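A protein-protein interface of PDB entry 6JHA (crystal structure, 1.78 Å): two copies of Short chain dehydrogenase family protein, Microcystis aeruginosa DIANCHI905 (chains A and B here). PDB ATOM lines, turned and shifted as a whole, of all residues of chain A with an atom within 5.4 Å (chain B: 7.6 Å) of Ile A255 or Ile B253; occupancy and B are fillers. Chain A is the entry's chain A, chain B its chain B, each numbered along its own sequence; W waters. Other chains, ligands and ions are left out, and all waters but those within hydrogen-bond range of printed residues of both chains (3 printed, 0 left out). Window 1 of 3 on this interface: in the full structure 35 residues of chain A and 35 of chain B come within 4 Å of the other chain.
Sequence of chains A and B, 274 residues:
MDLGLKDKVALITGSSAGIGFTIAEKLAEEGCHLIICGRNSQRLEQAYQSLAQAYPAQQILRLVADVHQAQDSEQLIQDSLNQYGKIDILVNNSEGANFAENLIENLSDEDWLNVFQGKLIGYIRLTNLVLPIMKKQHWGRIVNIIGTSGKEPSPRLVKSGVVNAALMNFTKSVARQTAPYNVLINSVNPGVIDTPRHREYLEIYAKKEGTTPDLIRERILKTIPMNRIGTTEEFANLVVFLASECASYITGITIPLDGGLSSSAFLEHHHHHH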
ATOM      1  N   SER A 187      27.699  17.206   5.761  1.00  0.00           N
ATOM      2  CA  SER A 187      29.052  16.724   5.603  1.00  0.00           C
ATOM      3  C   SER A 187      29.761  17.380   4.429  1.00  0.00           C
ATOM      4  O   SER A 187      29.141  17.823   3.468  1.00  0.00           O
ATOM      5  CB  SER A 187      29.078  15.203   5.490  1.00  0.00           C
ATOM      6  OG  SER A 187      28.467  14.737   4.294  1.00  0.00           O
ATOM      7  N   VAL A 188      31.088  17.467   4.531  1.00  0.00           N
ATOM      8  CA  VAL A 188      31.870  18.025   3.476  1.00  0.00           C
ATOM      9  C   VAL A 188      32.956  17.024   3.128  1.00  0.00           C
ATOM     10  O   VAL A 188      33.646  16.503   4.021  1.00  0.00           O
ATOM     11  CB  VAL A 188      32.500  19.377   3.869  1.00  0.00           C
ATOM     12  CG1 VAL A 188      33.361  19.920   2.747  1.00  0.00           C
ATOM     13  CG2 VAL A 188      31.423  20.368   4.244  1.00  0.00           C
ATOM     14  N   ASN A 189      33.125  16.796   1.839  1.00  0.00           N
ATOM     15  CA  ASN A 189      34.103  15.806   1.344  1.00  0.00           C
ATOM     16  C   ASN A 189      35.235  16.501   0.649  1.00  0.00           C
ATOM     17  O   ASN A 189      35.072  17.012  -0.453  1.00  0.00           O
ATOM     18  CB  ASN A 189      33.382  14.834   0.415  1.00  0.00           C
ATOM     19  CG  ASN A 189      33.090  13.518   1.077  1.00  0.00           C
ATOM     20  OD1 ASN A 189      32.166  13.409   1.903  1.00  0.00           O
ATOM     21  ND2 ASN A 189      33.925  12.511   0.787  1.00  0.00           N
ATOM     22  N   LEU A 238      33.654  27.064   3.427  1.00  0.00           N
ATOM     23  CA  LEU A 238      32.415  26.338   3.265  1.00  0.00           C
ATOM     24  C   LEU A 238      31.907  25.786   4.611  1.00  0.00           C
ATOM     25  O   LEU A 238      30.710  25.828   4.880  1.00  0.00           O
ATOM     26  CB  LEU A 238      32.528  25.234   2.230  1.00  0.00           C
ATOM     27  CG  LEU A 238      31.274  24.358   2.109  1.00  0.00           C
ATOM     28  CD1 LEU A 238      30.050  25.178   1.688  1.00  0.00           C
ATOM     29  CD2 LEU A 238      31.464  23.137   1.218  1.00  0.00           C
ATOM     30  N   LEU A 242      28.313  26.587   6.433  1.00  0.00           N
ATOM     31  CA  LEU A 242      27.378  25.579   6.861  1.00  0.00           C
ATOM     32  C   LEU A 242      27.098  25.684   8.369  1.00  0.00           C
ATOM     33  O   LEU A 242      26.024  25.327   8.788  1.00  0.00           O
ATOM     34  CB  LEU A 242      27.884  24.183   6.543  1.00  0.00           C
ATOM     35  CG  LEU A 242      27.858  23.834   5.051  1.00  0.00           C
ATOM     36  CD1 LEU A 242      28.549  22.525   4.779  1.00  0.00           C
ATOM     37  CD2 LEU A 242      26.392  23.815   4.627  1.00  0.00           C
ATOM     38  N   ILE A 253      22.912  17.017   3.901  1.00  0.00           N
ATOM     39  CA  ILE A 253      23.581  16.916   2.642  1.00  0.00           C
ATOM     40  C   ILE A 253      25.092  16.731   2.779  1.00  0.00           C
ATOM     41  O   ILE A 253      25.665  17.008   3.795  1.00  0.00           O
ATOM     42  CB  ILE A 253      23.228  18.079   1.747  1.00  0.00           C
ATOM     43  CG1 ILE A 253      23.930  19.360   2.164  1.00  0.00           C
ATOM     44  CG2 ILE A 253      21.702  18.145   1.561  1.00  0.00           C
ATOM     45  CD1 ILE A 253      23.743  20.499   1.223  1.00  0.00           C
ATOM     46  N   THR A 254      25.700  16.203   1.719  1.00  0.00           N
ATOM     47  CA  THR A 254      27.126  16.048   1.661  1.00  0.00           C
ATOM     48  C   THR A 254      27.623  16.816   0.475  1.00  0.00           C
ATOM     49  O   THR A 254      27.146  16.573  -0.622  1.00  0.00           O
ATOM     50  CB  THR A 254      27.513  14.573   1.529  1.00  0.00           C
ATOM     51  OG1 THR A 254      27.073  13.837   2.678  1.00  0.00           O
ATOM     52  CG2 THR A 254      29.030  14.440   1.378  1.00  0.00           C
ATOM     53  N   ILE A 255      28.579  17.736   0.678  1.00  0.00           N
ATOM     54  CA  ILE A 255      29.070  18.635  -0.361  1.00  0.00           C
ATOM     55  C   ILE A 255      30.548  18.319  -0.656  1.00  0.00           C
ATOM     56  O   ILE A 255      31.372  18.413   0.241  1.00  0.00           O
ATOM     57  CB  ILE A 255      28.966  20.098   0.075  1.00  0.00           C
ATOM     58  CG1 ILE A 255      27.499  20.434   0.473  1.00  0.00           C
ATOM     59  CG2 ILE A 255      29.492  21.022  -1.030  1.00  0.00           C
ATOM     60  CD1 ILE A 255      27.332  21.865   0.952  1.00  0.00           C
ATOM     61  N   PRO A 256      30.891  17.989  -1.920  1.00  0.00           N
ATOM     62  CA  PRO A 256      32.297  17.846  -2.323  1.00  0.00           C
ATOM     63  C   PRO A 256      32.984  19.214  -2.494  1.00  0.00           C
ATOM     64  O   PRO A 256      32.407  20.139  -3.119  1.00  0.00           O
ATOM     65  CB  PRO A 256      32.200  17.119  -3.682  1.00  0.00           C
ATOM     66  CG  PRO A 256      30.780  16.746  -3.859  1.00  0.00           C
ATOM     67  CD  PRO A 256      29.947  17.597  -2.973  1.00  0.00           C
ATOM     68  N   LEU A 257      34.175  19.351  -1.935  1.00  0.00           N
ATOM     69  CA  LEU A 257      34.919  20.592  -1.991  1.00  0.00           C
ATOM     70  C   LEU A 257      36.252  20.184  -2.552  1.00  0.00           C
ATOM     71  O   LEU A 257      37.195  19.853  -1.807  1.00  0.00           O
ATOM     72  CB  LEU A 257      35.003  21.242  -0.611  1.00  0.00           C
ATOM     73  CG  LEU A 257      35.349  22.744  -0.726  1.00  0.00           C
ATOM     74  CD1 LEU A 257      34.918  23.542   0.490  1.00  0.00           C
ATOM     75  CD2 LEU A 257      36.835  22.874  -0.910  1.00  0.00           C
ATOM     76  N   ASP A 258      36.331  20.171  -3.884  1.00  0.00           N
ATOM     77  CA  ASP A 258      37.335  19.320  -4.507  1.00  0.00           C
ATOM     78  C   ASP A 258      37.946  19.789  -5.829  1.00  0.00           C
ATOM     79  O   ASP A 258      38.585  18.982  -6.544  1.00  0.00           O
ATOM     80  CB  ASP A 258      36.694  17.950  -4.709  1.00  0.00           C
ATOM     81  CG  ASP A 258      35.601  17.951  -5.786  1.00  0.00           C
ATOM     82  OD1 ASP A 258      35.022  16.891  -5.952  1.00  0.00           O
ATOM     83  OD2 ASP A 258      35.295  18.981  -6.439  1.00  0.00           O
ATOM     84  N   SER A 262      34.969  15.626  -8.562  1.00  0.00           N
ATOM     85  CA  SER A 262      33.739  14.875  -8.652  1.00  0.00           C
ATOM     86  C   SER A 262      33.036  15.025 -10.005  1.00  0.00           C
ATOM     87  O   SER A 262      32.105  14.255 -10.291  1.00  0.00           O
ATOM     88  CB  SER A 262      32.795  15.204  -7.467  1.00  0.00           C
ATOM     89  OG  SER A 262      32.198  16.480  -7.662  1.00  0.00           O
ATOM     90  N   ILE B 142      28.917  30.771 -12.345  1.00  0.00           N
ATOM     91  CA  ILE B 142      27.597  30.505 -12.859  1.00  0.00           C
ATOM     92  C   ILE B 142      26.898  29.621 -11.826  1.00  0.00           C
ATOM     93  O   ILE B 142      27.471  28.601 -11.367  1.00  0.00           O
ATOM     94  CB  ILE B 142      27.625  29.814 -14.251  1.00  0.00           C
ATOM     95  CG1 ILE B 142      28.449  30.684 -15.237  1.00  0.00           C
ATOM     96  CG2 ILE B 142      26.218  29.537 -14.748  1.00  0.00           C
ATOM     97  CD1 ILE B 142      28.625  30.053 -16.576  1.00  0.00           C
ATOM     98  N   VAL B 143      25.746  30.067 -11.399  1.00  0.00           N
ATOM     99  CA  VAL B 143      24.920  29.298 -10.506  1.00  0.00           C
ATOM    100  C   VAL B 143      23.579  29.050 -11.194  1.00  0.00           C
ATOM    101  O   VAL B 143      22.824  30.000 -11.512  1.00  0.00           O
ATOM    102  CB  VAL B 143      24.717  29.961  -9.109  1.00  0.00           C
ATOM    103  CG1 VAL B 143      23.946  28.976  -8.205  1.00  0.00           C
ATOM    104  CG2 VAL B 143      26.021  30.351  -8.491  1.00  0.00           C
ATOM    105  N   ASN B 144      23.252  27.758 -11.383  1.00  0.00           N
ATOM    106  CA  ASN B 144      22.011  27.361 -12.012  1.00  0.00           C
ATOM    107  C   ASN B 144      20.954  27.013 -10.984  1.00  0.00           C
ATOM    108  O   ASN B 144      21.189  26.189 -10.112  1.00  0.00           O
ATOM    109  CB  ASN B 144      22.238  26.138 -12.893  1.00  0.00           C
ATOM    110  CG  ASN B 144      23.221  26.380 -14.018  1.00  0.00           C
ATOM    111  OD1 ASN B 144      23.154  27.366 -14.716  1.00  0.00           O
ATOM    112  ND2 ASN B 144      24.141  25.481 -14.188  1.00  0.00           N
ATOM    113  N   ILE B 146      17.967  25.022 -10.295  1.00  0.00           N
ATOM    114  CA  ILE B 146      17.381  23.870 -10.945  1.00  0.00           C
ATOM    115  C   ILE B 146      16.137  23.425 -10.203  1.00  0.00           C
ATOM    116  O   ILE B 146      15.092  23.994 -10.386  1.00  0.00           O
ATOM    117  CB  ILE B 146      18.468  22.799 -11.154  1.00  0.00           C
ATOM    118  CG1 ILE B 146      19.558  23.365 -12.087  1.00  0.00           C
ATOM    119  CG2 ILE B 146      17.904  21.549 -11.818  1.00  0.00           C
ATOM    120  CD1 ILE B 146      20.737  22.451 -12.356  1.00  0.00           C
ATOM    121  N   MET B 168      21.630  19.160 -14.413  1.00  0.00           N
ATOM    122  CA  MET B 168      22.644  18.715 -13.436  1.00  0.00           C
ATOM    123  C   MET B 168      23.841  18.044 -14.113  1.00  0.00           C
ATOM    124  O   MET B 168      25.006  18.245 -13.764  1.00  0.00           O
ATOM    125  CB  MET B 168      21.971  17.779 -12.391  1.00  0.00           C
ATOM    126  CG  MET B 168      20.942  18.496 -11.501  1.00  0.00           C
ATOM    127  SD  MET B 168      19.930  17.323 -10.529  1.00  0.00           S
ATOM    128  CE  MET B 168      21.227  16.555  -9.622  1.00  0.00           C
ATOM    129  N   THR B 171      25.883  20.738 -15.929  1.00  0.00           N
ATOM    130  CA  THR B 171      26.666  21.427 -14.923  1.00  0.00           C
ATOM    131  C   THR B 171      28.030  20.754 -14.703  1.00  0.00           C
ATOM    132  O   THR B 171      29.056  21.400 -14.707  1.00  0.00           O
ATOM    133  CB  THR B 171      25.861  21.553 -13.590  1.00  0.00           C
ATOM    134  OG1 THR B 171      24.694  22.356 -13.809  1.00  0.00           O
ATOM    135  CG2 THR B 171      26.744  22.171 -12.535  1.00  0.00           C
ATOM    136  N   LYS B 172      28.048  19.442 -14.592  1.00  0.00           N
ATOM    137  CA  LYS B 172      29.286  18.700 -14.375  1.00  0.00           C
ATOM    138  C   LYS B 172      30.201  18.780 -15.587  1.00  0.00           C
ATOM    139  O   LYS B 172      31.389  19.015 -15.455  1.00  0.00           O
ATOM    140  CB  LYS B 172      29.012  17.242 -14.048  1.00  0.00           C
ATOM    141  CG  LYS B 172      28.178  17.033 -12.810  1.00  0.00           C
ATOM    142  CD  LYS B 172      28.058  15.525 -12.505  1.00  0.00           C
ATOM    143  N   ALA B 175      31.536  22.447 -15.963  1.00  0.00           N
ATOM    144  CA  ALA B 175      32.495  22.679 -14.875  1.00  0.00           C
ATOM    145  C   ALA B 175      33.844  22.078 -15.128  1.00  0.00           C
ATOM    146  O   ALA B 175      34.868  22.736 -14.923  1.00  0.00           O
ATOM    147  CB  ALA B 175      31.927  22.269 -13.540  1.00  0.00           C
ATOM    148  N   ILE B 185      31.114  26.618 -11.915  1.00  0.00           N
ATOM    149  CA  ILE B 185      29.736  26.407 -12.274  1.00  0.00           C
ATOM    150  C   ILE B 185      29.115  25.362 -11.389  1.00  0.00           C
ATOM    151  O   ILE B 185      29.670  24.269 -11.264  1.00  0.00           O
ATOM    152  CB  ILE B 185      29.646  25.934 -13.739  1.00  0.00           C
ATOM    153  CG1 ILE B 185      30.375  26.969 -14.627  1.00  0.00           C
ATOM    154  CG2 ILE B 185      28.220  25.757 -14.102  1.00  0.00           C
ATOM    155  CD1 ILE B 185      30.764  26.499 -15.997  1.00  0.00           C
ATOM    156  N   ASN B 186      28.061  25.769 -10.693  1.00  0.00           N
ATOM    157  CA  ASN B 186      27.351  24.949  -9.741  1.00  0.00           C
ATOM    158  C   ASN B 186      25.863  25.103  -9.878  1.00  0.00           C
ATOM    159  O   ASN B 186      25.322  26.029 -10.528  1.00  0.00           O
ATOM    160  CB  ASN B 186      27.775  25.265  -8.311  1.00  0.00           C
ATOM    161  CG  ASN B 186      29.268  25.037  -8.069  1.00  0.00           C
ATOM    162  OD1 ASN B 186      29.757  23.899  -8.036  1.00  0.00           O
ATOM    163  ND2 ASN B 186      29.996  26.115  -7.912  1.00  0.00           N
ATOM    164  N   SER B 187      25.123  24.203  -9.258  1.00  0.00           N
ATOM    165  CA  SER B 187      23.674  24.370  -9.241  1.00  0.00           C
ATOM    166  C   SER B 187      23.124  24.220  -7.850  1.00  0.00           C
ATOM    167  O   SER B 187      23.743  23.553  -6.973  1.00  0.00           O
ATOM    168  CB  SER B 187      22.995  23.376 -10.162  1.00  0.00           C
ATOM    169  OG  SER B 187      23.383  22.063  -9.826  1.00  0.00           O
ATOM    170  N   VAL B 188      21.999  24.870  -7.634  1.00  0.00           N
ATOM    171  CA  VAL B 188      21.283  24.747  -6.383  1.00  0.00           C
ATOM    172  C   VAL B 188      19.882  24.246  -6.695  1.00  0.00           C
ATOM    173  O   VAL B 188      19.206  24.760  -7.571  1.00  0.00           O
ATOM    174  CB  VAL B 188      21.265  26.094  -5.646  1.00  0.00           C
ATOM    175  CG1 VAL B 188      20.526  25.986  -4.309  1.00  0.00           C
ATOM    176  CG2 VAL B 188      22.682  26.590  -5.424  1.00  0.00           C
ATOM    177  N   LEU B 238      22.930  30.856   0.052  1.00  0.00           N
ATOM    178  CA  LEU B 238      23.832  29.873  -0.563  1.00  0.00           C
ATOM    179  C   LEU B 238      24.267  30.300  -1.958  1.00  0.00           C
ATOM    180  O   LEU B 238      25.430  30.137  -2.311  1.00  0.00           O
ATOM    181  CB  LEU B 238      23.221  28.461  -0.593  1.00  0.00           C
ATOM    182  CG  LEU B 238      24.137  27.422  -1.275  1.00  0.00           C
ATOM    183  CD1 LEU B 238      25.389  27.208  -0.458  1.00  0.00           C
ATOM    184  CD2 LEU B 238      23.405  26.113  -1.499  1.00  0.00           C
ATOM    185  N   LEU B 242      28.111  30.804  -3.237  1.00  0.00           N
ATOM    186  CA  LEU B 242      28.671  30.122  -4.410  1.00  0.00           C
ATOM    187  C   LEU B 242      29.169  31.108  -5.456  1.00  0.00           C
ATOM    188  O   LEU B 242      30.133  30.772  -6.184  1.00  0.00           O
ATOM    189  CB  LEU B 242      27.697  29.154  -5.042  1.00  0.00           C
ATOM    190  CG  LEU B 242      27.327  27.929  -4.210  1.00  0.00           C
ATOM    191  CD1 LEU B 242      26.170  27.209  -4.874  1.00  0.00           C
ATOM    192  CD2 LEU B 242      28.493  26.999  -4.083  1.00  0.00           C
ATOM    193  N   TYR B 249      37.166  26.947  -4.608  1.00  0.00           N
ATOM    194  CA  TYR B 249      37.520  25.550  -4.870  1.00  0.00           C
ATOM    195  C   TYR B 249      36.293  24.654  -5.100  1.00  0.00           C
ATOM    196  O   TYR B 249      36.406  23.427  -5.089  1.00  0.00           O
ATOM    197  CB  TYR B 249      38.419  24.985  -3.769  1.00  0.00           C
ATOM    198  CG  TYR B 249      39.368  23.906  -4.245  1.00  0.00           C
ATOM    199  CD1 TYR B 249      39.383  22.657  -3.667  1.00  0.00           C
ATOM    200  CD2 TYR B 249      40.266  24.174  -5.286  1.00  0.00           C
ATOM    201  CE1 TYR B 249      40.292  21.678  -4.117  1.00  0.00           C
ATOM    202  CE2 TYR B 249      41.160  23.228  -5.745  1.00  0.00           C
ATOM    203  CZ  TYR B 249      41.143  21.975  -5.173  1.00  0.00           C
ATOM    204  OH  TYR B 249      42.077  21.042  -5.643  1.00  0.00           O
ATOM    205  N   ILE B 250      35.118  25.272  -5.271  1.00  0.00           N
ATOM    206  CA  ILE B 250      33.880  24.523  -5.421  1.00  0.00           C
ATOM    207  C   ILE B 250      33.382  24.655  -6.860  1.00  0.00           C
ATOM    208  O   ILE B 250      33.008  25.732  -7.286  1.00  0.00           O
ATOM    209  CB  ILE B 250      32.764  25.061  -4.474  1.00  0.00           C
ATOM    210  CG1 ILE B 250      33.203  24.933  -3.026  1.00  0.00           C
ATOM    211  CG2 ILE B 250      31.455  24.302  -4.653  1.00  0.00           C
ATOM    212  CD1 ILE B 250      32.215  25.606  -2.085  1.00  0.00           C
ATOM    213  N   THR B 251      33.304  23.534  -7.579  1.00  0.00           N
ATOM    214  CA  THR B 251      32.760  23.556  -8.914  1.00  0.00           C
ATOM    215  C   THR B 251      32.194  22.176  -9.301  1.00  0.00           C
ATOM    216  O   THR B 251      32.650  21.137  -8.807  1.00  0.00           O
ATOM    217  CB  THR B 251      33.798  24.099  -9.959  1.00  0.00           C
ATOM    218  OG1 THR B 251      33.067  24.490 -11.135  1.00  0.00           O
ATOM    219  CG2 THR B 251      34.858  23.077 -10.267  1.00  0.00           C
ATOM    220  N   GLY B 252      31.178  22.195 -10.139  1.00  0.00           N
ATOM    221  CA  GLY B 252      30.589  20.997 -10.758  1.00  0.00           C
ATOM    222  C   GLY B 252      29.588  20.288  -9.865  1.00  0.00           C
ATOM    223  O   GLY B 252      29.167  19.167 -10.155  1.00  0.00           O
ATOM    224  N   ILE B 253      29.152  20.944  -8.793  1.00  0.00           N
ATOM    225  CA  ILE B 253      28.253  20.261  -7.860  1.00  0.00           C
ATOM    226  C   ILE B 253      26.848  20.832  -7.870  1.00  0.00           C
ATOM    227  O   ILE B 253      26.636  21.959  -8.298  1.00  0.00           O
ATOM    228  CB  ILE B 253      28.859  20.243  -6.439  1.00  0.00           C
ATOM    229  CG1 ILE B 253      28.949  21.632  -5.884  1.00  0.00           C
ATOM    230  CG2 ILE B 253      30.241  19.561  -6.464  1.00  0.00           C
ATOM    231  CD1 ILE B 253      28.818  21.700  -4.403  1.00  0.00           C
ATOM    232  N   THR B 254      25.892  20.040  -7.388  1.00  0.00           N
ATOM    233  CA  THR B 254      24.510  20.468  -7.245  1.00  0.00           C
ATOM    234  C   THR B 254      24.150  20.277  -5.802  1.00  0.00           C
ATOM    235  O   THR B 254      24.319  19.180  -5.289  1.00  0.00           O
ATOM    236  CB  THR B 254      23.552  19.668  -8.147  1.00  0.00           C
ATOM    237  OG1 THR B 254      23.871  19.901  -9.534  1.00  0.00           O
ATOM    238  CG2 THR B 254      22.141  20.103  -7.913  1.00  0.00           C
ATOM    239  N   ILE B 255      23.707  21.340  -5.145  1.00  0.00           N
ATOM    240  CA  ILE B 255      23.424  21.329  -3.707  1.00  0.00           C
ATOM    241  C   ILE B 255      21.926  21.488  -3.481  1.00  0.00           C
ATOM    242  O   ILE B 255      21.342  22.494  -3.938  1.00  0.00           O
ATOM    243  CB  ILE B 255      24.150  22.501  -3.012  1.00  0.00           C
ATOM    244  CG1 ILE B 255      25.662  22.460  -3.266  1.00  0.00           C
ATOM    245  CG2 ILE B 255      23.907  22.496  -1.515  1.00  0.00           C
ATOM    246  CD1 ILE B 255      26.386  23.610  -2.618  1.00  0.00           C
ATOM    247  N   PRO B 256      21.273  20.518  -2.783  1.00  0.00           N
ATOM    248  CA  PRO B 256      19.918  20.685  -2.324  1.00  0.00           C
ATOM    249  C   PRO B 256      19.791  21.743  -1.227  1.00  0.00           C
ATOM    250  O   PRO B 256      20.555  21.737  -0.255  1.00  0.00           O
ATOM    251  CB  PRO B 256      19.566  19.309  -1.730  1.00  0.00           C
ATOM    252  CG  PRO B 256      20.614  18.399  -2.212  1.00  0.00           C
ATOM    253  CD  PRO B 256      21.825  19.242  -2.300  1.00  0.00           C
HETATM  254  O   HOH W   1      33.733  21.091  -5.412  1.00  0.00           O
HETATM  255  O   HOH W   2      41.045  18.456  -5.377  1.00  0.00           O
HETATM  256  O   HOH W   3      33.335  18.499  -8.430  1.00  0.00           O
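Ile A253 touches Ile B255, and with the chains exchanged Ile A255 touches Ile B253. Ile A253 touches Pro B256, and with the chains exchanged Pro A256 touches Ile B253. Of the 8 pairs that touch across the chains among the printed residues, 4 have their exchanged pair printed and touching as well.
Water W3 lies within hydrogen-bond range of OG of Ser A262 (2.4 Å), O of Thr B251 (2.8 Å) and OD2 of Asp A258 (2.8 Å). Water W2 bridges O of Asp A258 and OH of Tyr B249. Water W1 lies within hydrogen-bond range of the backbone carbonyl oxygen of Pro A256, the side-chain carboxylate of Asp A258 and the backbone NH of Thr B251.
CG2 of Ile B255 touches CD1 of Ile A253 (3.4 Å). Pro B256 touches Ile A253. Ile B253 touches Ile A255. Pro A256 touches Ile B253 (CG to CG2, 3.9 Å). Leu A257 touches Tyr B249 (CD2 to CD1, 3.8 Å). Leu A257 touches Ile B250 (CG to CG1, 3.8 Å). Ser A262 touches Ile B253 (OG to CG2, 3.8 Å).
Of the printed residues of chain B, Ile A255 touches Ile B253 (3.5 Å). Of the printed residues of chain B, Pro A256 touches Ile B253. Of the printed residues of chain B, Leu A257 touches Tyr B249 and Ile B250. Asn B144 touches none of the printed residues of chain A. Of the printed residues of chain A, Tyr B249 touches Leu A257 (3.8 Å) and Asp A258 (3.5 Å). Of chain A, only Ile A255 (3.5 Å), Pro A256 (3.9 Å) and Ser A262 (3.8 Å) come within 4 Å of Ile B253. Of the printed residues of chain A, Ile B255 touches Ile A253. The nearest residue of chain A that does not touch Ile B253 is Asp A258 (5.1 Å). The nearest printed residue of chain B that does not touch Leu A257 is Ile B253 (6.0 Å).
O of Ile B253 lies within hydrogen-bond range of N of Ser B187, 2.9 Å away. The side-chain amide nitrogen of Asn B186 lies within hydrogen-bond range of the backbone carbonyl oxygen of Ile B250, at 3.1 Å. N of Ile A255 is in hydrogen-bond range of O of Ser A187. The backbone carbonyl oxygen (O) of Ile A253 lies within hydrogen-bond range of the backbone NH (N) of Ser A187 (2.8 Å). The backbone NH (N) of Ser A262 sits at hydrogen-bond distance from the side-chain carboxylate (OD1) of Asp A258 (2.9 Å). The backbone NH (N) of Leu A257 sits at hydrogen-bond distance from the backbone carbonyl oxygen (O) of Asn A189 (2.9 Å).
The backbone NH (N) of Asp A258 lies within hydrogen-bond range of the backbone carbonyl oxygen (O) of Tyr B249 (3.5 Å).
Printed residues of chain A that touch a printed residue of chain B: Ile A253, Ile A255, Pro A256, Leu A257, Asp A258 and Ser A262. Hydrophobic or aromatic side chains of chain A that line the printed part of chain B: Ile A253, Ile A255, Pro A256 and Leu A257. Along chain B the printed residues that touch a printed residue of chain A span positions 249 to 256. Among the printed residues, 8 pairs touch across the chains.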
